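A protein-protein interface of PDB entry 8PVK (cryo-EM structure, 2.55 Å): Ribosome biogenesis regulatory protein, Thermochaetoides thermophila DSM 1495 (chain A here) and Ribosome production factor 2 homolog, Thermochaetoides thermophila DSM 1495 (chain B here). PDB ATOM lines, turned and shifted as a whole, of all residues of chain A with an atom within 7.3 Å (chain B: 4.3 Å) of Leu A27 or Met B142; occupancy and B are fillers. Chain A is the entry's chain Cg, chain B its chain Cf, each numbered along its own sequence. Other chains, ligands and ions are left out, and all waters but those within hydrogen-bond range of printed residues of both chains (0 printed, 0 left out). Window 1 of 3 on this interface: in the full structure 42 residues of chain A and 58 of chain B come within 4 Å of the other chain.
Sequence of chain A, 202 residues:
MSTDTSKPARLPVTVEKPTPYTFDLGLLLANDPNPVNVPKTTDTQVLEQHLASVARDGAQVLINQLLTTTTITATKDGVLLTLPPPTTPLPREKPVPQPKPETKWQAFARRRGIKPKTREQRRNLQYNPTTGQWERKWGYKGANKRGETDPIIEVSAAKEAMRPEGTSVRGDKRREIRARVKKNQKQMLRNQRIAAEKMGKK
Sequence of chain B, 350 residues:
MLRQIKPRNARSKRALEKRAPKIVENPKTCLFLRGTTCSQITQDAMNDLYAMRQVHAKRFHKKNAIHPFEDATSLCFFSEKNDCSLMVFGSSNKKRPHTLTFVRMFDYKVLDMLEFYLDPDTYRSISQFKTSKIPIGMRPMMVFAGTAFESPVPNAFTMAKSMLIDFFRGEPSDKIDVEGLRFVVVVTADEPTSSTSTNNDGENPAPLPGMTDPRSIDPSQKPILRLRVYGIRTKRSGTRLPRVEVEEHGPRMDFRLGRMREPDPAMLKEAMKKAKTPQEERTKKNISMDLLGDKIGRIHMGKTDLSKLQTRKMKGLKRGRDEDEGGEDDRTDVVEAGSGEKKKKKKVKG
N of Phe B144 sits at hydrogen-bond distance from O of Ala A30 (3.0 Å). The backbone NH (N) of Met B142 is in hydrogen-bond range of the backbone carbonyl oxygen (O) of Leu A28 (3.0 Å). O of Met B142 sits at hydrogen-bond distance from N of Ala A30 (2.9 Å).
Of the 19 printed residues of chain A, 8 touch a printed residue of chain B. Printed residues of chain A that touch a printed residue of chain B: Leu A27, Leu A28, Leu A29, Ala A30, Asn A31, Gly A58, Leu A62 and Leu A90. Hydrophobic or aromatic side chains of chain A that line the printed part of chain B: Leu A27, Leu A28, Leu A29, Leu A62 and Leu A90. Of the 9 printed residues of chain B, 6 touch a printed residue of chain A. Printed residues of chain B that touch a printed residue of chain A: Met B141, Met B142, Val B143, Phe B144, Ile B165 and Arg B169. Hydrophobic or aromatic side chains of chain B that line the printed part of chain A: Met B141, Met B142, Val B143, Phe B144 and Ile B165. Among the printed residues, 15 pairs touch across the chains.
Leu A25 touches none of the printed residues of chain B. Of the printed residues of chain B, Leu A27 touches Met B142 (3.4 Å) and Arg B169 (3.4 Å). Printed residues of chain B within 4 Å of Leu A28: Met B141 and Met B142. Of the printed residues of chain B, Leu A90 touches Ile B165 (3.7 Å) and Arg B169 (3.3 Å). Of the printed residues of chain A, Met B142 touches Leu A27, Leu A28, Leu A29 and Ala A30. Of the printed residues of chain A, Phe B144 touches Leu A29 (3.6 Å), Ala A30 (3.0 Å) and Asn A31 (3.6 Å). Of the printed residues of chain A, Ile B165 touches Leu A29 and Leu A90. Phe B168 touches none of the printed residues of chain A. The nearest printed residue of chain B that does not touch Leu A27 is Ile B165 (4.003 Å).
The backbone carbonyl oxygen (O) of Met B141 lies within hydrogen-bond range of the backbone NH (N) of Val B185, at 2.9 Å. OD2 of Asp A24 lies within hydrogen-bond range of N of Leu A27, 3.3 Å away. N of Asp A24 is in hydrogen-bond range of O of Leu A29, at 2.9 Å. The backbone carbonyl oxygen (O) of Val B185 sits at hydrogen-bond distance from the backbone NH (N) of Val B143 (2.9 Å).
Among the printed residues, pairs that only touch across the chains: Leu A27 with Met B142 (3.4 Å), Leu A27 with Arg B169 (3.4 Å), Leu A28 with Met B141 (3.4 Å), Leu A29 with Met B142 (3.4 Å), Leu A29 with Phe B144 (3.6 Å), Leu A29 with Ile B165 (3.7 Å), Ala A30 with Val B143 (3.3 Å), Asn A31 with Phe B144 (3.6 Å), Gly A58 with Val B143 (3.99 Å), Leu A62 with Met B141 (3.7 Å), Leu A90 with Ile B165 (3.7 Å) and Leu A90 with Arg B169 (3.3 Å).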
ATOM      1  N   PHE A  23      12.861   0.253  -5.160  1.00  0.00           N
ATOM      2  CA  PHE A  23      13.953   1.213  -5.133  1.00  0.00           C
ATOM      3  C   PHE A  23      14.405   1.506  -3.714  1.00  0.00           C
ATOM      4  O   PHE A  23      13.633   1.404  -2.758  1.00  0.00           O
ATOM      5  CB  PHE A  23      13.557   2.529  -5.807  1.00  0.00           C
ATOM      6  CG  PHE A  23      13.385   2.412  -7.282  1.00  0.00           C
ATOM      7  CD1 PHE A  23      14.488   2.435  -8.116  1.00  0.00           C
ATOM      8  CD2 PHE A  23      12.127   2.271  -7.837  1.00  0.00           C
ATOM      9  CE1 PHE A  23      14.340   2.321  -9.478  1.00  0.00           C
ATOM     10  CE2 PHE A  23      11.973   2.156  -9.199  1.00  0.00           C
ATOM     11  CZ  PHE A  23      13.082   2.182 -10.018  1.00  0.00           C
ATOM     12  N   ASP A  24      15.681   1.877  -3.602  1.00  0.00           N
ATOM     13  CA  ASP A  24      16.244   2.502  -2.406  1.00  0.00           C
ATOM     14  C   ASP A  24      17.174   3.559  -3.005  1.00  0.00           C
ATOM     15  O   ASP A  24      18.324   3.270  -3.347  1.00  0.00           O
ATOM     16  CB  ASP A  24      16.964   1.482  -1.518  1.00  0.00           C
ATOM     17  CG  ASP A  24      17.708   2.105  -0.315  1.00  0.00           C
ATOM     18  OD1 ASP A  24      17.871   1.369   0.679  1.00  0.00           O
ATOM     19  OD2 ASP A  24      18.121   3.284  -0.307  1.00  0.00           O
ATOM     20  N   LEU A  25      16.661   4.781  -3.141  1.00  0.00           N
ATOM     21  CA  LEU A  25      17.405   5.843  -3.803  1.00  0.00           C
ATOM     22  C   LEU A  25      18.541   6.401  -2.953  1.00  0.00           C
ATOM     23  O   LEU A  25      19.395   7.115  -3.489  1.00  0.00           O
ATOM     24  CB  LEU A  25      16.451   6.970  -4.206  1.00  0.00           C
ATOM     25  CG  LEU A  25      15.326   6.550  -5.155  1.00  0.00           C
ATOM     26  CD1 LEU A  25      14.491   7.748  -5.563  1.00  0.00           C
ATOM     27  CD2 LEU A  25      15.881   5.842  -6.380  1.00  0.00           C
ATOM     28  N   GLY A  26      18.565   6.108  -1.651  1.00  0.00           N
ATOM     29  CA  GLY A  26      19.701   6.507  -0.836  1.00  0.00           C
ATOM     30  C   GLY A  26      20.976   5.785  -1.224  1.00  0.00           C
ATOM     31  O   GLY A  26      22.065   6.367  -1.198  1.00  0.00           O
ATOM     32  N   LEU A  27      20.862   4.510  -1.586  1.00  0.00           N
ATOM     33  CA  LEU A  27      21.991   3.721  -2.054  1.00  0.00           C
ATOM     34  C   LEU A  27      22.042   3.610  -3.571  1.00  0.00           C
ATOM     35  O   LEU A  27      22.911   2.904  -4.094  1.00  0.00           O
ATOM     36  CB  LEU A  27      21.949   2.323  -1.436  1.00  0.00           C
ATOM     37  CG  LEU A  27      22.095   2.275   0.084  1.00  0.00           C
ATOM     38  CD1 LEU A  27      22.032   0.844   0.587  1.00  0.00           C
ATOM     39  CD2 LEU A  27      23.395   2.940   0.498  1.00  0.00           C
ATOM     40  N   LEU A  28      21.138   4.303  -4.275  1.00  0.00           N
ATOM     41  CA  LEU A  28      20.980   4.207  -5.731  1.00  0.00           C
ATOM     42  C   LEU A  28      20.773   2.760  -6.169  1.00  0.00           C
ATOM     43  O   LEU A  28      21.344   2.297  -7.159  1.00  0.00           O
ATOM     44  CB  LEU A  28      22.167   4.838  -6.467  1.00  0.00           C
ATOM     45  CG  LEU A  28      22.674   6.185  -5.951  1.00  0.00           C
ATOM     46  CD1 LEU A  28      24.030   6.501  -6.556  1.00  0.00           C
ATOM     47  CD2 LEU A  28      21.677   7.286  -6.257  1.00  0.00           C
ATOM     48  N   LEU A  29      19.953   2.032  -5.416  1.00  0.00           N
ATOM     49  CA  LEU A  29      19.741   0.608  -5.623  1.00  0.00           C
ATOM     50  C   LEU A  29      18.370   0.374  -6.239  1.00  0.00           C
ATOM     51  O   LEU A  29      17.364   0.890  -5.740  1.00  0.00           O
ATOM     52  CB  LEU A  29      19.864  -0.152  -4.302  1.00  0.00           C
ATOM     53  CG  LEU A  29      19.257  -1.553  -4.238  1.00  0.00           C
ATOM     54  CD1 LEU A  29      20.076  -2.537  -5.052  1.00  0.00           C
ATOM     55  CD2 LEU A  29      19.136  -2.010  -2.795  1.00  0.00           C
ATOM     56  N   ALA A  30      18.334  -0.399  -7.319  1.00  0.00           N
ATOM     57  CA  ALA A  30      17.094  -0.807  -7.960  1.00  0.00           C
ATOM     58  C   ALA A  30      17.015  -2.326  -7.950  1.00  0.00           C
ATOM     59  O   ALA A  30      17.941  -3.002  -8.408  1.00  0.00           O
ATOM     60  CB  ALA A  30      17.008  -0.275  -9.392  1.00  0.00           C
ATOM     61  N   ASN A  31      15.914  -2.856  -7.429  1.00  0.00           N
ATOM     62  CA  ASN A  31      15.694  -4.292  -7.340  1.00  0.00           C
ATOM     63  C   ASN A  31      14.656  -4.701  -8.373  1.00  0.00           C
ATOM     64  O   ASN A  31      13.560  -4.126  -8.426  1.00  0.00           O
ATOM     65  CB  ASN A  31      15.231  -4.694  -5.939  1.00  0.00           C
ATOM     66  CG  ASN A  31      16.140  -4.166  -4.852  1.00  0.00           C
ATOM     67  OD1 ASN A  31      16.105  -2.983  -4.517  1.00  0.00           O
ATOM     68  ND2 ASN A  31      16.960  -5.043  -4.291  1.00  0.00           N
ATOM     69  N   GLY A  58      17.263  -1.876 -16.299  1.00  0.00           N
ATOM     70  CA  GLY A  58      17.425  -1.477 -14.908  1.00  0.00           C
ATOM     71  C   GLY A  58      17.967  -0.068 -14.754  1.00  0.00           C
ATOM     72  O   GLY A  58      17.453   0.723 -13.955  1.00  0.00           O
ATOM     73  N   LEU A  62      15.988   3.170 -13.201  1.00  0.00           N
ATOM     74  CA  LEU A  62      16.620   3.878 -12.087  1.00  0.00           C
ATOM     75  C   LEU A  62      16.828   5.357 -12.399  1.00  0.00           C
ATOM     76  O   LEU A  62      16.594   6.217 -11.539  1.00  0.00           O
ATOM     77  CB  LEU A  62      17.948   3.211 -11.735  1.00  0.00           C
ATOM     78  CG  LEU A  62      18.662   3.675 -10.464  1.00  0.00           C
ATOM     79  CD1 LEU A  62      17.695   3.804  -9.299  1.00  0.00           C
ATOM     80  CD2 LEU A  62      19.786   2.714 -10.123  1.00  0.00           C
ATOM     81  N   LEU A  83      18.415  13.069  -2.035  1.00  0.00           N
ATOM     82  CA  LEU A  83      18.064  11.667  -1.891  1.00  0.00           C
ATOM     83  C   LEU A  83      17.412  11.399  -0.539  1.00  0.00           C
ATOM     84  O   LEU A  83      17.752  12.040   0.461  1.00  0.00           O
ATOM     85  CB  LEU A  83      19.306  10.783  -2.028  1.00  0.00           C
ATOM     86  CG  LEU A  83      20.172  10.971  -3.272  1.00  0.00           C
ATOM     87  CD1 LEU A  83      21.409  10.096  -3.183  1.00  0.00           C
ATOM     88  CD2 LEU A  83      19.378  10.666  -4.531  1.00  0.00           C
ATOM     89  N   PRO A  84      16.474  10.458  -0.485  1.00  0.00           N
ATOM     90  CA  PRO A  84      15.939  10.014   0.802  1.00  0.00           C
ATOM     91  C   PRO A  84      16.971   9.196   1.556  1.00  0.00           C
ATOM     92  O   PRO A  84      17.934   8.699   0.951  1.00  0.00           O
ATOM     93  CB  PRO A  84      14.728   9.158   0.400  1.00  0.00           C
ATOM     94  CG  PRO A  84      15.065   8.663  -0.958  1.00  0.00           C
ATOM     95  CD  PRO A  84      15.818   9.782  -1.618  1.00  0.00           C
ATOM     96  N   PRO A  85      16.831   9.061   2.874  1.00  0.00           N
ATOM     97  CA  PRO A  85      17.749   8.203   3.618  1.00  0.00           C
ATOM     98  C   PRO A  85      17.580   6.754   3.207  1.00  0.00           C
ATOM     99  O   PRO A  85      16.488   6.336   2.779  1.00  0.00           O
ATOM    100  CB  PRO A  85      17.338   8.428   5.081  1.00  0.00           C
ATOM    101  CG  PRO A  85      15.953   8.969   5.015  1.00  0.00           C
ATOM    102  CD  PRO A  85      15.906   9.781   3.765  1.00  0.00           C
ATOM    103  N   PRO A  86      18.648   5.956   3.288  1.00  0.00           N
ATOM    104  CA  PRO A  86      18.558   4.549   2.871  1.00  0.00           C
ATOM    105  C   PRO A  86      17.619   3.747   3.760  1.00  0.00           C
ATOM    106  O   PRO A  86      17.526   3.974   4.968  1.00  0.00           O
ATOM    107  CB  PRO A  86      20.003   4.051   2.991  1.00  0.00           C
ATOM    108  CG  PRO A  86      20.843   5.287   2.970  1.00  0.00           C
ATOM    109  CD  PRO A  86      20.024   6.334   3.652  1.00  0.00           C
ATOM    110  N   THR A  87      16.917   2.795   3.140  1.00  0.00           N
ATOM    111  CA  THR A  87      15.950   1.962   3.837  1.00  0.00           C
ATOM    112  C   THR A  87      16.303   0.482   3.843  1.00  0.00           C
ATOM    113  O   THR A  87      15.657  -0.282   4.571  1.00  0.00           O
ATOM    114  CB  THR A  87      14.551   2.131   3.223  1.00  0.00           C
ATOM    115  OG1 THR A  87      14.573   1.715   1.853  1.00  0.00           O
ATOM    116  CG2 THR A  87      14.102   3.582   3.303  1.00  0.00           C
ATOM    117  N   THR A  88      17.288   0.054   3.062  1.00  0.00           N
ATOM    118  CA  THR A  88      17.673  -1.352   3.052  1.00  0.00           C
ATOM    119  C   THR A  88      18.421  -1.690   4.336  1.00  0.00           C
ATOM    120  O   THR A  88      19.411  -1.026   4.664  1.00  0.00           O
ATOM    121  CB  THR A  88      18.543  -1.665   1.836  1.00  0.00           C
ATOM    122  OG1 THR A  88      17.790  -1.443   0.638  1.00  0.00           O
ATOM    123  CG2 THR A  88      19.007  -3.113   1.870  1.00  0.00           C
ATOM    124  N   PRO A  89      17.980  -2.696   5.092  1.00  0.00           N
ATOM    125  CA  PRO A  89      18.663  -3.033   6.349  1.00  0.00           C
ATOM    126  C   PRO A  89      20.011  -3.692   6.088  1.00  0.00           C
ATOM    127  O   PRO A  89      20.102  -4.701   5.386  1.00  0.00           O
ATOM    128  CB  PRO A  89      17.689  -3.998   7.038  1.00  0.00           C
ATOM    129  CG  PRO A  89      16.380  -3.827   6.316  1.00  0.00           C
ATOM    130  CD  PRO A  89      16.746  -3.478   4.912  1.00  0.00           C
ATOM    131  N   LEU A  90      21.059  -3.108   6.661  1.00  0.00           N
ATOM    132  CA  LEU A  90      22.407  -3.649   6.620  1.00  0.00           C
ATOM    133  C   LEU A  90      23.009  -3.611   8.016  1.00  0.00           C
ATOM    134  O   LEU A  90      22.704  -2.705   8.800  1.00  0.00           O
ATOM    135  CB  LEU A  90      23.295  -2.863   5.643  1.00  0.00           C
ATOM    136  CG  LEU A  90      22.965  -3.045   4.161  1.00  0.00           C
ATOM    137  CD1 LEU A  90      23.582  -1.935   3.342  1.00  0.00           C
ATOM    138  CD2 LEU A  90      23.438  -4.403   3.668  1.00  0.00           C
ATOM    139  N   PRO B 140      29.123   4.073  -7.827  1.00  0.00           N
ATOM    140  CA  PRO B 140      28.200   3.633  -8.872  1.00  0.00           C
ATOM    141  C   PRO B 140      26.848   3.232  -8.298  1.00  0.00           C
ATOM    142  O   PRO B 140      26.701   2.959  -7.104  1.00  0.00           O
ATOM    143  CB  PRO B 140      28.922   2.419  -9.471  1.00  0.00           C
ATOM    144  CG  PRO B 140      29.646   1.832  -8.305  1.00  0.00           C
ATOM    145  CD  PRO B 140      30.018   2.985  -7.391  1.00  0.00           C
ATOM    146  N   MET B 141      25.852   3.208  -9.175  1.00  0.00           N
ATOM    147  CA  MET B 141      24.545   2.711  -8.774  1.00  0.00           C
ATOM    148  C   MET B 141      24.511   1.191  -8.890  1.00  0.00           C
ATOM    149  O   MET B 141      25.385   0.572  -9.494  1.00  0.00           O
ATOM    150  CB  MET B 141      23.434   3.351  -9.604  1.00  0.00           C
ATOM    151  CG  MET B 141      23.663   4.813  -9.933  1.00  0.00           C
ATOM    152  SD  MET B 141      22.380   5.476 -11.009  1.00  0.00           S
ATOM    153  CE  MET B 141      22.710   4.580 -12.515  1.00  0.00           C
ATOM    154  N   MET B 142      23.497   0.582  -8.279  1.00  0.00           N
ATOM    155  CA  MET B 142      23.396  -0.870  -8.215  1.00  0.00           C
ATOM    156  C   MET B 142      22.048  -1.334  -8.744  1.00  0.00           C
ATOM    157  O   MET B 142      21.014  -0.722  -8.462  1.00  0.00           O
ATOM    158  CB  MET B 142      23.590  -1.380  -6.781  1.00  0.00           C
ATOM    159  CG  MET B 142      24.842  -0.862  -6.092  1.00  0.00           C
ATOM    160  SD  MET B 142      24.976  -1.416  -4.385  1.00  0.00           S
ATOM    161  CE  MET B 142      24.789   0.136  -3.514  1.00  0.00           C
ATOM    162  N   VAL B 143      22.070  -2.419  -9.515  1.00  0.00           N
ATOM    163  CA  VAL B 143      20.867  -3.078 -10.013  1.00  0.00           C
ATOM    164  C   VAL B 143      20.992  -4.565  -9.715  1.00  0.00           C
ATOM    165  O   VAL B 143      21.945  -5.214 -10.165  1.00  0.00           O
ATOM    166  CB  VAL B 143      20.654  -2.844 -11.519  1.00  0.00           C
ATOM    167  CG1 VAL B 143      19.571  -3.767 -12.052  1.00  0.00           C
ATOM    168  CG2 VAL B 143      20.290  -1.395 -11.790  1.00  0.00           C
ATOM    169  N   PHE B 144      20.036  -5.102  -8.963  1.00  0.00           N
ATOM    170  CA  PHE B 144      19.979  -6.523  -8.640  1.00  0.00           C
ATOM    171  C   PHE B 144      18.779  -7.126  -9.356  1.00  0.00           C
ATOM    172  O   PHE B 144      17.654  -6.638  -9.206  1.00  0.00           O
ATOM    173  CB  PHE B 144      19.883  -6.738  -7.130  1.00  0.00           C
ATOM    174  CG  PHE B 144      21.208  -6.681  -6.428  1.00  0.00           C
ATOM    175  CD1 PHE B 144      21.837  -5.467  -6.211  1.00  0.00           C
ATOM    176  CD2 PHE B 144      21.826  -7.838  -5.988  1.00  0.00           C
ATOM    177  CE1 PHE B 144      23.057  -5.407  -5.569  1.00  0.00           C
ATOM    178  CE2 PHE B 144      23.046  -7.785  -5.343  1.00  0.00           C
ATOM    179  CZ  PHE B 144      23.662  -6.569  -5.134  1.00  0.00           C
ATOM    180  N   ILE B 165      25.822  -5.325  -1.809  1.00  0.00           N
ATOM    181  CA  ILE B 165      25.313  -3.992  -1.501  1.00  0.00           C
ATOM    182  C   ILE B 165      26.235  -3.291  -0.512  1.00  0.00           C
ATOM    183  O   ILE B 165      26.554  -2.106  -0.671  1.00  0.00           O
ATOM    184  CB  ILE B 165      23.865  -4.081  -0.976  1.00  0.00           C
ATOM    185  CG1 ILE B 165      22.896  -4.362  -2.123  1.00  0.00           C
ATOM    186  CG2 ILE B 165      23.447  -2.799  -0.278  1.00  0.00           C
ATOM    187  CD1 ILE B 165      21.496  -4.683  -1.661  1.00  0.00           C
ATOM    188  N   PHE B 168      29.555  -2.308  -2.422  1.00  0.00           N
ATOM    189  CA  PHE B 168      29.402  -1.175  -3.322  1.00  0.00           C
ATOM    190  C   PHE B 168      28.596  -0.040  -2.696  1.00  0.00           C
ATOM    191  O   PHE B 168      28.094   0.826  -3.420  1.00  0.00           O
ATOM    192  CB  PHE B 168      28.759  -1.630  -4.632  1.00  0.00           C
ATOM    193  CG  PHE B 168      29.637  -2.528  -5.458  1.00  0.00           C
ATOM    194  CD1 PHE B 168      30.725  -2.015  -6.145  1.00  0.00           C
ATOM    195  CD2 PHE B 168      29.373  -3.885  -5.550  1.00  0.00           C
ATOM    196  CE1 PHE B 168      31.533  -2.838  -6.907  1.00  0.00           C
ATOM    197  CE2 PHE B 168      30.178  -4.713  -6.311  1.00  0.00           C
ATOM    198  CZ  PHE B 168      31.259  -4.189  -6.989  1.00  0.00           C
ATOM    199  N   ARG B 169      28.449  -0.047  -1.366  1.00  0.00           N
ATOM    200  CA  ARG B 169      27.727   1.015  -0.671  1.00  0.00           C
ATOM    201  C   ARG B 169      28.399   2.370  -0.848  1.00  0.00           C
ATOM    202  O   ARG B 169      27.724   3.373  -1.103  1.00  0.00           O
ATOM    203  CB  ARG B 169      27.612   0.677   0.817  1.00  0.00           C
ATOM    204  CG  ARG B 169      26.802   1.672   1.639  1.00  0.00           C
ATOM    205  CD  ARG B 169      26.665   1.209   3.084  1.00  0.00           C
ATOM    206  NE  ARG B 169      25.970   2.183   3.918  1.00  0.00           N
ATOM    207  CZ  ARG B 169      24.653   2.254   4.062  1.00  0.00           C
ATOM    208  NH1 ARG B 169      23.845   1.399   3.460  1.00  0.00           N
ATOM    209  NH2 ARG B 169      24.136   3.203   4.835  1.00  0.00           N
ATOM    210  N   VAL B 185      26.406  -1.180 -11.506  1.00  0.00           N
ATOM    211  CA  VAL B 185      26.861  -2.536 -11.237  1.00  0.00           C
ATOM    212  C   VAL B 185      25.625  -3.420 -11.143  1.00  0.00           C
ATOM    213  O   VAL B 185      24.746  -3.183 -10.307  1.00  0.00           O
ATOM    214  CB  VAL B 185      27.694  -2.601  -9.947  1.00  0.00           C
ATOM    215  CG1 VAL B 185      27.870  -4.033  -9.497  1.00  0.00           C
ATOM    216  CG2 VAL B 185      29.043  -1.938 -10.158  1.00  0.00           C
